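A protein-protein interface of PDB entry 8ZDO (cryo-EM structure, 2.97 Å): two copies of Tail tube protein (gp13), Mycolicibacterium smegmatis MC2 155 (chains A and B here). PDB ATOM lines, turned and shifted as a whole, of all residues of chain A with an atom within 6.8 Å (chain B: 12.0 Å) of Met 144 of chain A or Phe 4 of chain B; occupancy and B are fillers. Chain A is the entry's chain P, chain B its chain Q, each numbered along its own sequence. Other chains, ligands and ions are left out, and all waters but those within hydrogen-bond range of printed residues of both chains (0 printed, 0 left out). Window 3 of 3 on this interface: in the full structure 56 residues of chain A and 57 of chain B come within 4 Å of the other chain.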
ATOM      1  N   ILE A  16      31.128  15.541 -18.708  1.00  0.00           N
ATOM      2  CA  ILE A  16      30.968  14.307 -19.465  1.00  0.00           C
ATOM      3  C   ILE A  16      29.858  14.511 -20.486  1.00  0.00           C
ATOM      4  O   ILE A  16      28.726  14.853 -20.124  1.00  0.00           O
ATOM      5  CB  ILE A  16      30.661  13.116 -18.546  1.00  0.00           C
ATOM      6  CG1 ILE A  16      31.763  12.957 -17.500  1.00  0.00           C
ATOM      7  CG2 ILE A  16      30.510  11.845 -19.359  1.00  0.00           C
ATOM      8  CD1 ILE A  16      31.387  12.056 -16.354  1.00  0.00           C
ATOM      9  N   ALA A  17      30.181  14.294 -21.760  1.00  0.00           N
ATOM     10  CA  ALA A  17      29.229  14.480 -22.844  1.00  0.00           C
ATOM     11  C   ALA A  17      28.724  13.130 -23.321  1.00  0.00           C
ATOM     12  O   ALA A  17      29.527  12.324 -23.814  1.00  0.00           O
ATOM     13  CB  ALA A  17      29.873  15.234 -23.999  1.00  0.00           C
ATOM     14  N   PRO A  18      27.428  12.845 -23.229  1.00  0.00           N
ATOM     15  CA  PRO A  18      26.933  11.534 -23.668  1.00  0.00           C
ATOM     16  C   PRO A  18      26.987  11.400 -25.180  1.00  0.00           C
ATOM     17  O   PRO A  18      25.978  11.573 -25.868  1.00  0.00           O
ATOM     18  CB  PRO A  18      25.494  11.508 -23.145  1.00  0.00           C
ATOM     19  CG  PRO A  18      25.100  12.940 -23.067  1.00  0.00           C
ATOM     20  CD  PRO A  18      26.342  13.730 -22.776  1.00  0.00           C
ATOM     21  N   LEU A  19      28.179  11.095 -25.699  1.00  0.00           N
ATOM     22  CA  LEU A  19      28.391  11.113 -27.142  1.00  0.00           C
ATOM     23  C   LEU A  19      27.524  10.084 -27.850  1.00  0.00           C
ATOM     24  O   LEU A  19      26.954  10.371 -28.909  1.00  0.00           O
ATOM     25  CB  LEU A  19      29.867  10.882 -27.458  1.00  0.00           C
ATOM     26  CG  LEU A  19      30.787  12.053 -27.122  1.00  0.00           C
ATOM     27  CD1 LEU A  19      32.179  11.803 -27.667  1.00  0.00           C
ATOM     28  CD2 LEU A  19      30.216  13.346 -27.672  1.00  0.00           C
ATOM     29  N   ASN A  20      27.416   8.878 -27.297  1.00  0.00           N
ATOM     30  CA  ASN A  20      26.550   7.857 -27.879  1.00  0.00           C
ATOM     31  C   ASN A  20      25.721   7.226 -26.776  1.00  0.00           C
ATOM     32  O   ASN A  20      26.275   6.672 -25.829  1.00  0.00           O
ATOM     33  CB  ASN A  20      27.363   6.792 -28.615  1.00  0.00           C
ATOM     34  CG  ASN A  20      26.517   5.968 -29.559  1.00  0.00           C
ATOM     35  OD1 ASN A  20      25.303   6.152 -29.647  1.00  0.00           O
ATOM     36  ND2 ASN A  20      27.153   5.050 -30.273  1.00  0.00           N
ATOM     37  N   LEU A  21      24.402   7.283 -26.906  1.00  0.00           N
ATOM     38  CA  LEU A  21      23.512   6.812 -25.857  1.00  0.00           C
ATOM     39  C   LEU A  21      22.568   5.752 -26.402  1.00  0.00           C
ATOM     40  O   LEU A  21      22.190   5.779 -27.576  1.00  0.00           O
ATOM     41  CB  LEU A  21      22.718   7.979 -25.256  1.00  0.00           C
ATOM     42  CG  LEU A  21      21.872   7.737 -24.007  1.00  0.00           C
ATOM     43  CD1 LEU A  21      21.834   8.999 -23.198  1.00  0.00           C
ATOM     44  CD2 LEU A  21      20.456   7.322 -24.360  1.00  0.00           C
ATOM     45  N   THR A  22      22.193   4.810 -25.539  1.00  0.00           N
ATOM     46  CA  THR A  22      21.227   3.785 -25.894  1.00  0.00           C
ATOM     47  C   THR A  22      20.331   3.472 -24.704  1.00  0.00           C
ATOM     48  O   THR A  22      20.728   3.606 -23.540  1.00  0.00           O
ATOM     49  CB  THR A  22      21.907   2.501 -26.397  1.00  0.00           C
ATOM     50  OG1 THR A  22      20.908   1.534 -26.744  1.00  0.00           O
ATOM     51  CG2 THR A  22      22.814   1.922 -25.349  1.00  0.00           C
ATOM     52  N   LEU A  44      31.646  -3.019 -19.804  1.00  0.00           N
ATOM     53  CA  LEU A  44      30.215  -2.755 -19.890  1.00  0.00           C
ATOM     54  C   LEU A  44      29.479  -4.086 -19.973  1.00  0.00           C
ATOM     55  O   LEU A  44      29.577  -4.796 -20.978  1.00  0.00           O
ATOM     56  CB  LEU A  44      29.909  -1.871 -21.093  1.00  0.00           C
ATOM     57  CG  LEU A  44      28.564  -1.145 -21.075  1.00  0.00           C
ATOM     58  CD1 LEU A  44      28.330  -0.489 -19.728  1.00  0.00           C
ATOM     59  CD2 LEU A  44      28.509  -0.119 -22.188  1.00  0.00           C
ATOM     60  N   VAL A 142      22.131   4.006 -20.944  1.00  0.00           N
ATOM     61  CA  VAL A 142      23.585   4.028 -20.830  1.00  0.00           C
ATOM     62  C   VAL A 142      24.164   4.836 -21.982  1.00  0.00           C
ATOM     63  O   VAL A 142      23.811   4.619 -23.145  1.00  0.00           O
ATOM     64  CB  VAL A 142      24.174   2.606 -20.765  1.00  0.00           C
ATOM     65  CG1 VAL A 142      23.860   1.815 -22.010  1.00  0.00           C
ATOM     66  CG2 VAL A 142      25.679   2.668 -20.545  1.00  0.00           C
ATOM     67  N   GLY A 143      25.030   5.789 -21.651  1.00  0.00           N
ATOM     68  CA  GLY A 143      25.699   6.600 -22.642  1.00  0.00           C
ATOM     69  C   GLY A 143      27.201   6.503 -22.468  1.00  0.00           C
ATOM     70  O   GLY A 143      27.701   6.233 -21.375  1.00  0.00           O
ATOM     71  N   MET A 144      27.916   6.725 -23.561  1.00  0.00           N
ATOM     72  CA  MET A 144      29.361   6.607 -23.609  1.00  0.00           C
ATOM     73  C   MET A 144      29.949   7.905 -24.133  1.00  0.00           C
ATOM     74  O   MET A 144      29.480   8.444 -25.145  1.00  0.00           O
ATOM     75  CB  MET A 144      29.795   5.437 -24.491  1.00  0.00           C
ATOM     76  CG  MET A 144      31.297   5.240 -24.555  1.00  0.00           C
ATOM     77  SD  MET A 144      31.770   3.886 -25.641  1.00  0.00           S
ATOM     78  CE  MET A 144      31.211   4.522 -27.216  1.00  0.00           C
ATOM     79  N   ASP A 145      30.955   8.401 -23.418  1.00  0.00           N
ATOM     80  CA  ASP A 145      31.791   9.520 -23.837  1.00  0.00           C
ATOM     81  C   ASP A 145      33.172   8.958 -24.138  1.00  0.00           C
ATOM     82  O   ASP A 145      33.863   8.486 -23.231  1.00  0.00           O
ATOM     83  CB  ASP A 145      31.858  10.587 -22.748  1.00  0.00           C
ATOM     84  CG  ASP A 145      32.631  11.817 -23.180  1.00  0.00           C
ATOM     85  OD1 ASP A 145      32.961  11.931 -24.378  1.00  0.00           O
ATOM     86  OD2 ASP A 145      32.910  12.675 -22.317  1.00  0.00           O
ATOM     87  N   ASP A 146      33.566   8.995 -25.407  1.00  0.00           N
ATOM     88  CA  ASP A 146      34.858   8.472 -25.838  1.00  0.00           C
ATOM     89  C   ASP A 146      35.888   9.589 -25.745  1.00  0.00           C
ATOM     90  O   ASP A 146      35.842  10.553 -26.515  1.00  0.00           O
ATOM     91  CB  ASP A 146      34.770   7.923 -27.258  1.00  0.00           C
ATOM     92  CG  ASP A 146      34.496   6.434 -27.292  1.00  0.00           C
ATOM     93  OD1 ASP A 146      34.822   5.748 -26.302  1.00  0.00           O
ATOM     94  OD2 ASP A 146      33.957   5.950 -28.308  1.00  0.00           O
ATOM     95  N   PRO A 151      36.912   5.233 -22.601  1.00  0.00           N
ATOM     96  CA  PRO A 151      35.503   5.634 -22.547  1.00  0.00           C
ATOM     97  C   PRO A 151      34.985   5.766 -21.126  1.00  0.00           C
ATOM     98  O   PRO A 151      35.415   5.064 -20.209  1.00  0.00           O
ATOM     99  CB  PRO A 151      34.789   4.501 -23.289  1.00  0.00           C
ATOM    100  CG  PRO A 151      35.679   3.327 -23.111  1.00  0.00           C
ATOM    101  CD  PRO A 151      37.078   3.869 -23.129  1.00  0.00           C
ATOM    102  N   ILE A 152      34.041   6.684 -20.958  1.00  0.00           N
ATOM    103  CA  ILE A 152      33.285   6.840 -19.723  1.00  0.00           C
ATOM    104  C   ILE A 152      31.851   6.427 -20.013  1.00  0.00           C
ATOM    105  O   ILE A 152      31.182   7.040 -20.853  1.00  0.00           O
ATOM    106  CB  ILE A 152      33.342   8.281 -19.195  1.00  0.00           C
ATOM    107  CG1 ILE A 152      34.789   8.733 -19.018  1.00  0.00           C
ATOM    108  CG2 ILE A 152      32.580   8.400 -17.889  1.00  0.00           C
ATOM    109  CD1 ILE A 152      34.919  10.133 -18.477  1.00  0.00           C
ATOM    110  N   TRP A 153      31.385   5.384 -19.334  1.00  0.00           N
ATOM    111  CA  TRP A 153      30.010   4.920 -19.454  1.00  0.00           C
ATOM    112  C   TRP A 153      29.227   5.473 -18.274  1.00  0.00           C
ATOM    113  O   TRP A 153      29.432   5.049 -17.134  1.00  0.00           O
ATOM    114  CB  TRP A 153      29.941   3.396 -19.483  1.00  0.00           C
ATOM    115  CG  TRP A 153      30.823   2.777 -20.504  1.00  0.00           C
ATOM    116  CD1 TRP A 153      30.821   3.020 -21.843  1.00  0.00           C
ATOM    117  CD2 TRP A 153      31.841   1.800 -20.275  1.00  0.00           C
ATOM    118  NE1 TRP A 153      31.778   2.260 -22.464  1.00  0.00           N
ATOM    119  CE2 TRP A 153      32.419   1.501 -21.522  1.00  0.00           C
ATOM    120  CE3 TRP A 153      32.320   1.150 -19.136  1.00  0.00           C
ATOM    121  CZ2 TRP A 153      33.451   0.581 -21.662  1.00  0.00           C
ATOM    122  CZ3 TRP A 153      33.345   0.238 -19.277  1.00  0.00           C
ATOM    123  CH2 TRP A 153      33.899  -0.038 -20.530  1.00  0.00           C
ATOM    124  N   LEU A 154      28.342   6.422 -18.542  1.00  0.00           N
ATOM    125  CA  LEU A 154      27.459   6.965 -17.522  1.00  0.00           C
ATOM    126  C   LEU A 154      26.044   6.493 -17.810  1.00  0.00           C
ATOM    127  O   LEU A 154      25.558   6.618 -18.936  1.00  0.00           O
ATOM    128  CB  LEU A 154      27.548   8.492 -17.469  1.00  0.00           C
ATOM    129  CG  LEU A 154      26.923   9.409 -18.518  1.00  0.00           C
ATOM    130  CD1 LEU A 154      26.995  10.825 -18.000  1.00  0.00           C
ATOM    131  CD2 LEU A 154      27.628   9.305 -19.859  1.00  0.00           C
ATOM    132  N   THR B   2      31.176  -6.233 -23.611  1.00  0.00           N
ATOM    133  CA  THR B   2      30.577  -5.979 -24.914  1.00  0.00           C
ATOM    134  C   THR B   2      30.682  -4.500 -25.267  1.00  0.00           C
ATOM    135  O   THR B   2      30.454  -3.636 -24.421  1.00  0.00           O
ATOM    136  CB  THR B   2      29.101  -6.411 -24.951  1.00  0.00           C
ATOM    137  OG1 THR B   2      28.962  -7.693 -24.325  1.00  0.00           O
ATOM    138  CG2 THR B   2      28.609  -6.503 -26.382  1.00  0.00           C
ATOM    139  N   ASP B   3      31.031  -4.208 -26.517  1.00  0.00           N
ATOM    140  CA  ASP B   3      31.187  -2.826 -26.932  1.00  0.00           C
ATOM    141  C   ASP B   3      29.827  -2.157 -27.122  1.00  0.00           C
ATOM    142  O   ASP B   3      28.781  -2.808 -27.221  1.00  0.00           O
ATOM    143  CB  ASP B   3      32.010  -2.729 -28.218  1.00  0.00           C
ATOM    144  CG  ASP B   3      31.412  -3.526 -29.355  1.00  0.00           C
ATOM    145  OD1 ASP B   3      31.094  -4.713 -29.143  1.00  0.00           O
ATOM    146  OD2 ASP B   3      31.263  -2.965 -30.460  1.00  0.00           O
ATOM    147  N   PHE B   4      29.866  -0.824 -27.174  1.00  0.00           N
ATOM    148  CA  PHE B   4      28.639  -0.040 -27.195  1.00  0.00           C
ATOM    149  C   PHE B   4      27.830  -0.295 -28.459  1.00  0.00           C
ATOM    150  O   PHE B   4      26.599  -0.362 -28.408  1.00  0.00           O
ATOM    151  CB  PHE B   4      28.968   1.444 -27.058  1.00  0.00           C
ATOM    152  CG  PHE B   4      27.897   2.235 -26.379  1.00  0.00           C
ATOM    153  CD1 PHE B   4      27.767   2.209 -25.004  1.00  0.00           C
ATOM    154  CD2 PHE B   4      27.010   2.993 -27.118  1.00  0.00           C
ATOM    155  CE1 PHE B   4      26.780   2.932 -24.380  1.00  0.00           C
ATOM    156  CE2 PHE B   4      26.021   3.714 -26.498  1.00  0.00           C
ATOM    157  CZ  PHE B   4      25.907   3.685 -25.129  1.00  0.00           C
ATOM    158  N   TYR B   5      28.500  -0.423 -29.607  1.00  0.00           N
ATOM    159  CA  TYR B   5      27.777  -0.668 -30.851  1.00  0.00           C
ATOM    160  C   TYR B   5      27.043  -2.001 -30.815  1.00  0.00           C
ATOM    161  O   TYR B   5      25.884  -2.092 -31.234  1.00  0.00           O
ATOM    162  CB  TYR B   5      28.736  -0.618 -32.038  1.00  0.00           C
ATOM    163  CG  TYR B   5      29.070   0.782 -32.493  1.00  0.00           C
ATOM    164  CD1 TYR B   5      28.422   1.882 -31.947  1.00  0.00           C
ATOM    165  CD2 TYR B   5      30.023   1.003 -33.477  1.00  0.00           C
ATOM    166  CE1 TYR B   5      28.722   3.165 -32.364  1.00  0.00           C
ATOM    167  CE2 TYR B   5      30.328   2.283 -33.900  1.00  0.00           C
ATOM    168  CZ  TYR B   5      29.674   3.359 -33.341  1.00  0.00           C
ATOM    169  OH  TYR B   5      29.975   4.635 -33.758  1.00  0.00           O
ATOM    170  N   THR B   6      27.701  -3.048 -30.315  1.00  0.00           N
ATOM    171  CA  THR B   6      27.047  -4.346 -30.212  1.00  0.00           C
ATOM    172  C   THR B   6      25.893  -4.308 -29.221  1.00  0.00           C
ATOM    173  O   THR B   6      24.847  -4.923 -29.457  1.00  0.00           O
ATOM    174  CB  THR B   6      28.061  -5.416 -29.814  1.00  0.00           C
ATOM    175  OG1 THR B   6      29.208  -5.327 -30.666  1.00  0.00           O
ATOM    176  CG2 THR B   6      27.451  -6.800 -29.943  1.00  0.00           C
ATOM    177  N   ILE B   7      26.061  -3.598 -28.104  1.00  0.00           N
ATOM    178  CA  ILE B   7      24.975  -3.492 -27.132  1.00  0.00           C
ATOM    179  C   ILE B   7      23.791  -2.741 -27.732  1.00  0.00           C
ATOM    180  O   ILE B   7      22.630  -3.078 -27.477  1.00  0.00           O
ATOM    181  CB  ILE B   7      25.477  -2.826 -25.838  1.00  0.00           C
ATOM    182  CG1 ILE B   7      26.479  -3.737 -25.129  1.00  0.00           C
ATOM    183  CG2 ILE B   7      24.321  -2.505 -24.908  1.00  0.00           C
ATOM    184  CD1 ILE B   7      27.024  -3.161 -23.846  1.00  0.00           C
ATOM    185  N   LYS B   8      24.066  -1.720 -28.545  1.00  0.00           N
ATOM    186  CA  LYS B   8      22.992  -0.932 -29.141  1.00  0.00           C
ATOM    187  C   LYS B   8      22.266  -1.710 -30.232  1.00  0.00           C
ATOM    188  O   LYS B   8      21.042  -1.604 -30.358  1.00  0.00           O
ATOM    189  CB  LYS B   8      23.556   0.374 -29.697  1.00  0.00           C
ATOM    190  CG  LYS B   8      22.509   1.429 -29.990  1.00  0.00           C
ATOM    191  CD  LYS B   8      23.141   2.678 -30.570  1.00  0.00           C
ATOM    192  CE  LYS B   8      22.091   3.708 -30.940  1.00  0.00           C
ATOM    193  NZ  LYS B   8      21.354   4.197 -29.748  1.00  0.00           N
ATOM    194  N   ASP B   9      23.007  -2.486 -31.025  1.00  0.00           N
ATOM    195  CA  ASP B   9      22.477  -3.332 -32.104  1.00  0.00           C
ATOM    196  C   ASP B   9      21.365  -2.640 -32.892  1.00  0.00           C
ATOM    197  O   ASP B   9      20.298  -3.199 -33.148  1.00  0.00           O
ATOM    198  CB  ASP B   9      22.024  -4.697 -31.570  1.00  0.00           C
ATOM    199  CG  ASP B   9      21.007  -4.599 -30.443  1.00  0.00           C
ATOM    200  OD1 ASP B   9      19.908  -4.048 -30.653  1.00  0.00           O
ATOM    201  OD2 ASP B   9      21.314  -5.080 -29.332  1.00  0.00           O
ATOM    202  N   ALA B  10      21.637  -1.404 -33.296  1.00  0.00           N
ATOM    203  CA  ALA B  10      20.672  -0.627 -34.057  1.00  0.00           C
ATOM    204  C   ALA B  10      20.641  -1.073 -35.513  1.00  0.00           C
ATOM    205  O   ALA B  10      21.679  -1.372 -36.108  1.00  0.00           O
ATOM    206  CB  ALA B  10      21.008   0.861 -33.974  1.00  0.00           C
ATOM    207  N   GLN B  11      19.439  -1.119 -36.084  1.00  0.00           N
ATOM    208  CA  GLN B  11      19.242  -1.440 -37.493  1.00  0.00           C
ATOM    209  C   GLN B  11      18.528  -0.279 -38.165  1.00  0.00           C
ATOM    210  O   GLN B  11      17.431   0.104 -37.746  1.00  0.00           O
ATOM    211  CB  GLN B  11      18.435  -2.729 -37.670  1.00  0.00           C
ATOM    212  CG  GLN B  11      19.176  -4.000 -37.305  1.00  0.00           C
ATOM    213  CD  GLN B  11      18.807  -4.508 -35.931  1.00  0.00           C
ATOM    214  OE1 GLN B  11      17.757  -4.163 -35.392  1.00  0.00           O
ATOM    215  NE2 GLN B  11      19.668  -5.338 -35.356  1.00  0.00           N
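The side-chain amino group of Lys 8 of chain B lies within hydrogen-bond range of the backbone carbonyl oxygen of Leu 21 of chain A. N of Thr 2 of chain B lies within hydrogen-bond range of O of Leu 44 of chain A.
Among the printed residues, pairs that only touch across the chains: Asn 20 of chain A with Phe 4 of chain B (3.0 Å), Asn 20 of chain A with Tyr 5 of chain B (3.2 Å), Leu 21 of chain A with Phe 4 of chain B (3.9 Å), Thr 22 of chain A with Phe 4 of chain B (3.6 Å), Thr 22 of chain A with Lys 8 of chain B (3.6 Å), Leu 44 of chain A with Phe 4 of chain B (3.7 Å), Leu 44 of chain A with Ile 7 of chain B (3.8 Å), Val 142 of chain A with Phe 4 of chain B (3.0 Å), Gly 143 of chain A with Phe 4 of chain B (3.8 Å) and Met 144 of chain A with Phe 4 of chain B (3.8 Å).
No residue of chain B comes within 4 Å of Pro 18 of chain A. No residue of chain B comes within 4 Å of Leu 19 of chain A. Of chain B, only Phe 4 (3.6 Å) and Lys 8 (3.6 Å) come within 4 Å of Thr 22 of chain A. Leu 44 of chain A touches just these residues of chain B: Thr 2, Phe 4 and Ile 7. Of chain B, only Phe 4 (3.0 Å) comes within 4 Å of Val 142 of chain A. Gly 143 of chain A touches one residue of chain B. Of chain B, only Phe 4 (3.8 Å) comes within 4 Å of Met 144 of chain A. No residue of chain B comes within 4 Å of Asp 145 of chain A. No residue of chain B comes within 4 Å of Asp 146 of chain A. No residue of chain B comes within 4 Å of Pro 151 of chain A. Ile 152 of chain A touches none of the printed residues of chain B. No residue of chain B comes within 4 Å of Trp 153 of chain A. No residue of chain B comes within 4 Å of Leu 154 of chain A. Of the printed residues of chain A, Thr 2 of chain B touches Leu 44 (3.4 Å). Of the printed residues of chain A, Phe 4 of chain B touches Asn 20, Leu 21, Thr 22, Leu 44, Val 142, Gly 143 and Met 144. Printed residues of chain A within 4 Å of Tyr 5 of chain B: Asn 20. Printed residues of chain A within 4 Å of Ile 7 of chain B: Leu 44 (3.8 Å). Of the printed residues of chain A, Lys 8 of chain B touches Leu 21 and Thr 22. Asp 9 of chain B touches none of the printed residues of chain A. Ala 10 of chain B touches none of the printed residues of chain A. The nearest residue of chain A that does not touch Phe 4 of chain B is Trp 153 of chain A (4.5 Å).
Of the 10 printed residues of chain B, 5 touch a printed residue of chain A. Hydrophobic or aromatic side chains of chain B that line the printed part of chain A: Phe 4, Tyr 5 and Ile 7. Of the 17 printed residues of chain A, 7 touch a printed residue of chain B. Hydrophobic or aromatic side chains of chain A that line the printed part of chain B: Leu 44, Val 142 and Met 144. Among the printed residues, 12 pairs touch across the chains. Among the printed residues, no Asp or Glu carboxylate lies within 4 Å of a Lys or Arg side-chain nitrogen of the other chain.
No position is printed for both chains.
The backbone NH (N) of Leu 19 of chain A sits at hydrogen-bond distance from the backbone carbonyl oxygen (O) of Met 144 of chain A, 3.0 Å away. The backbone carbonyl oxygen of Asn 20 of chain A is in hydrogen-bond range of the backbone NH of Met 144 of chain A (2.8 Å). O of Val 142 of chain A is in hydrogen-bond range of N of Thr 22 of chain A. N of Gly 143 of chain A is in hydrogen-bond range of O of Leu 154 of chain A (2.9 Å). The side-chain sulfur (SD) of Met 144 of chain A sits at hydrogen-bond distance from the indole nitrogen (NE1) of Trp 153 of chain A (3.6 Å).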
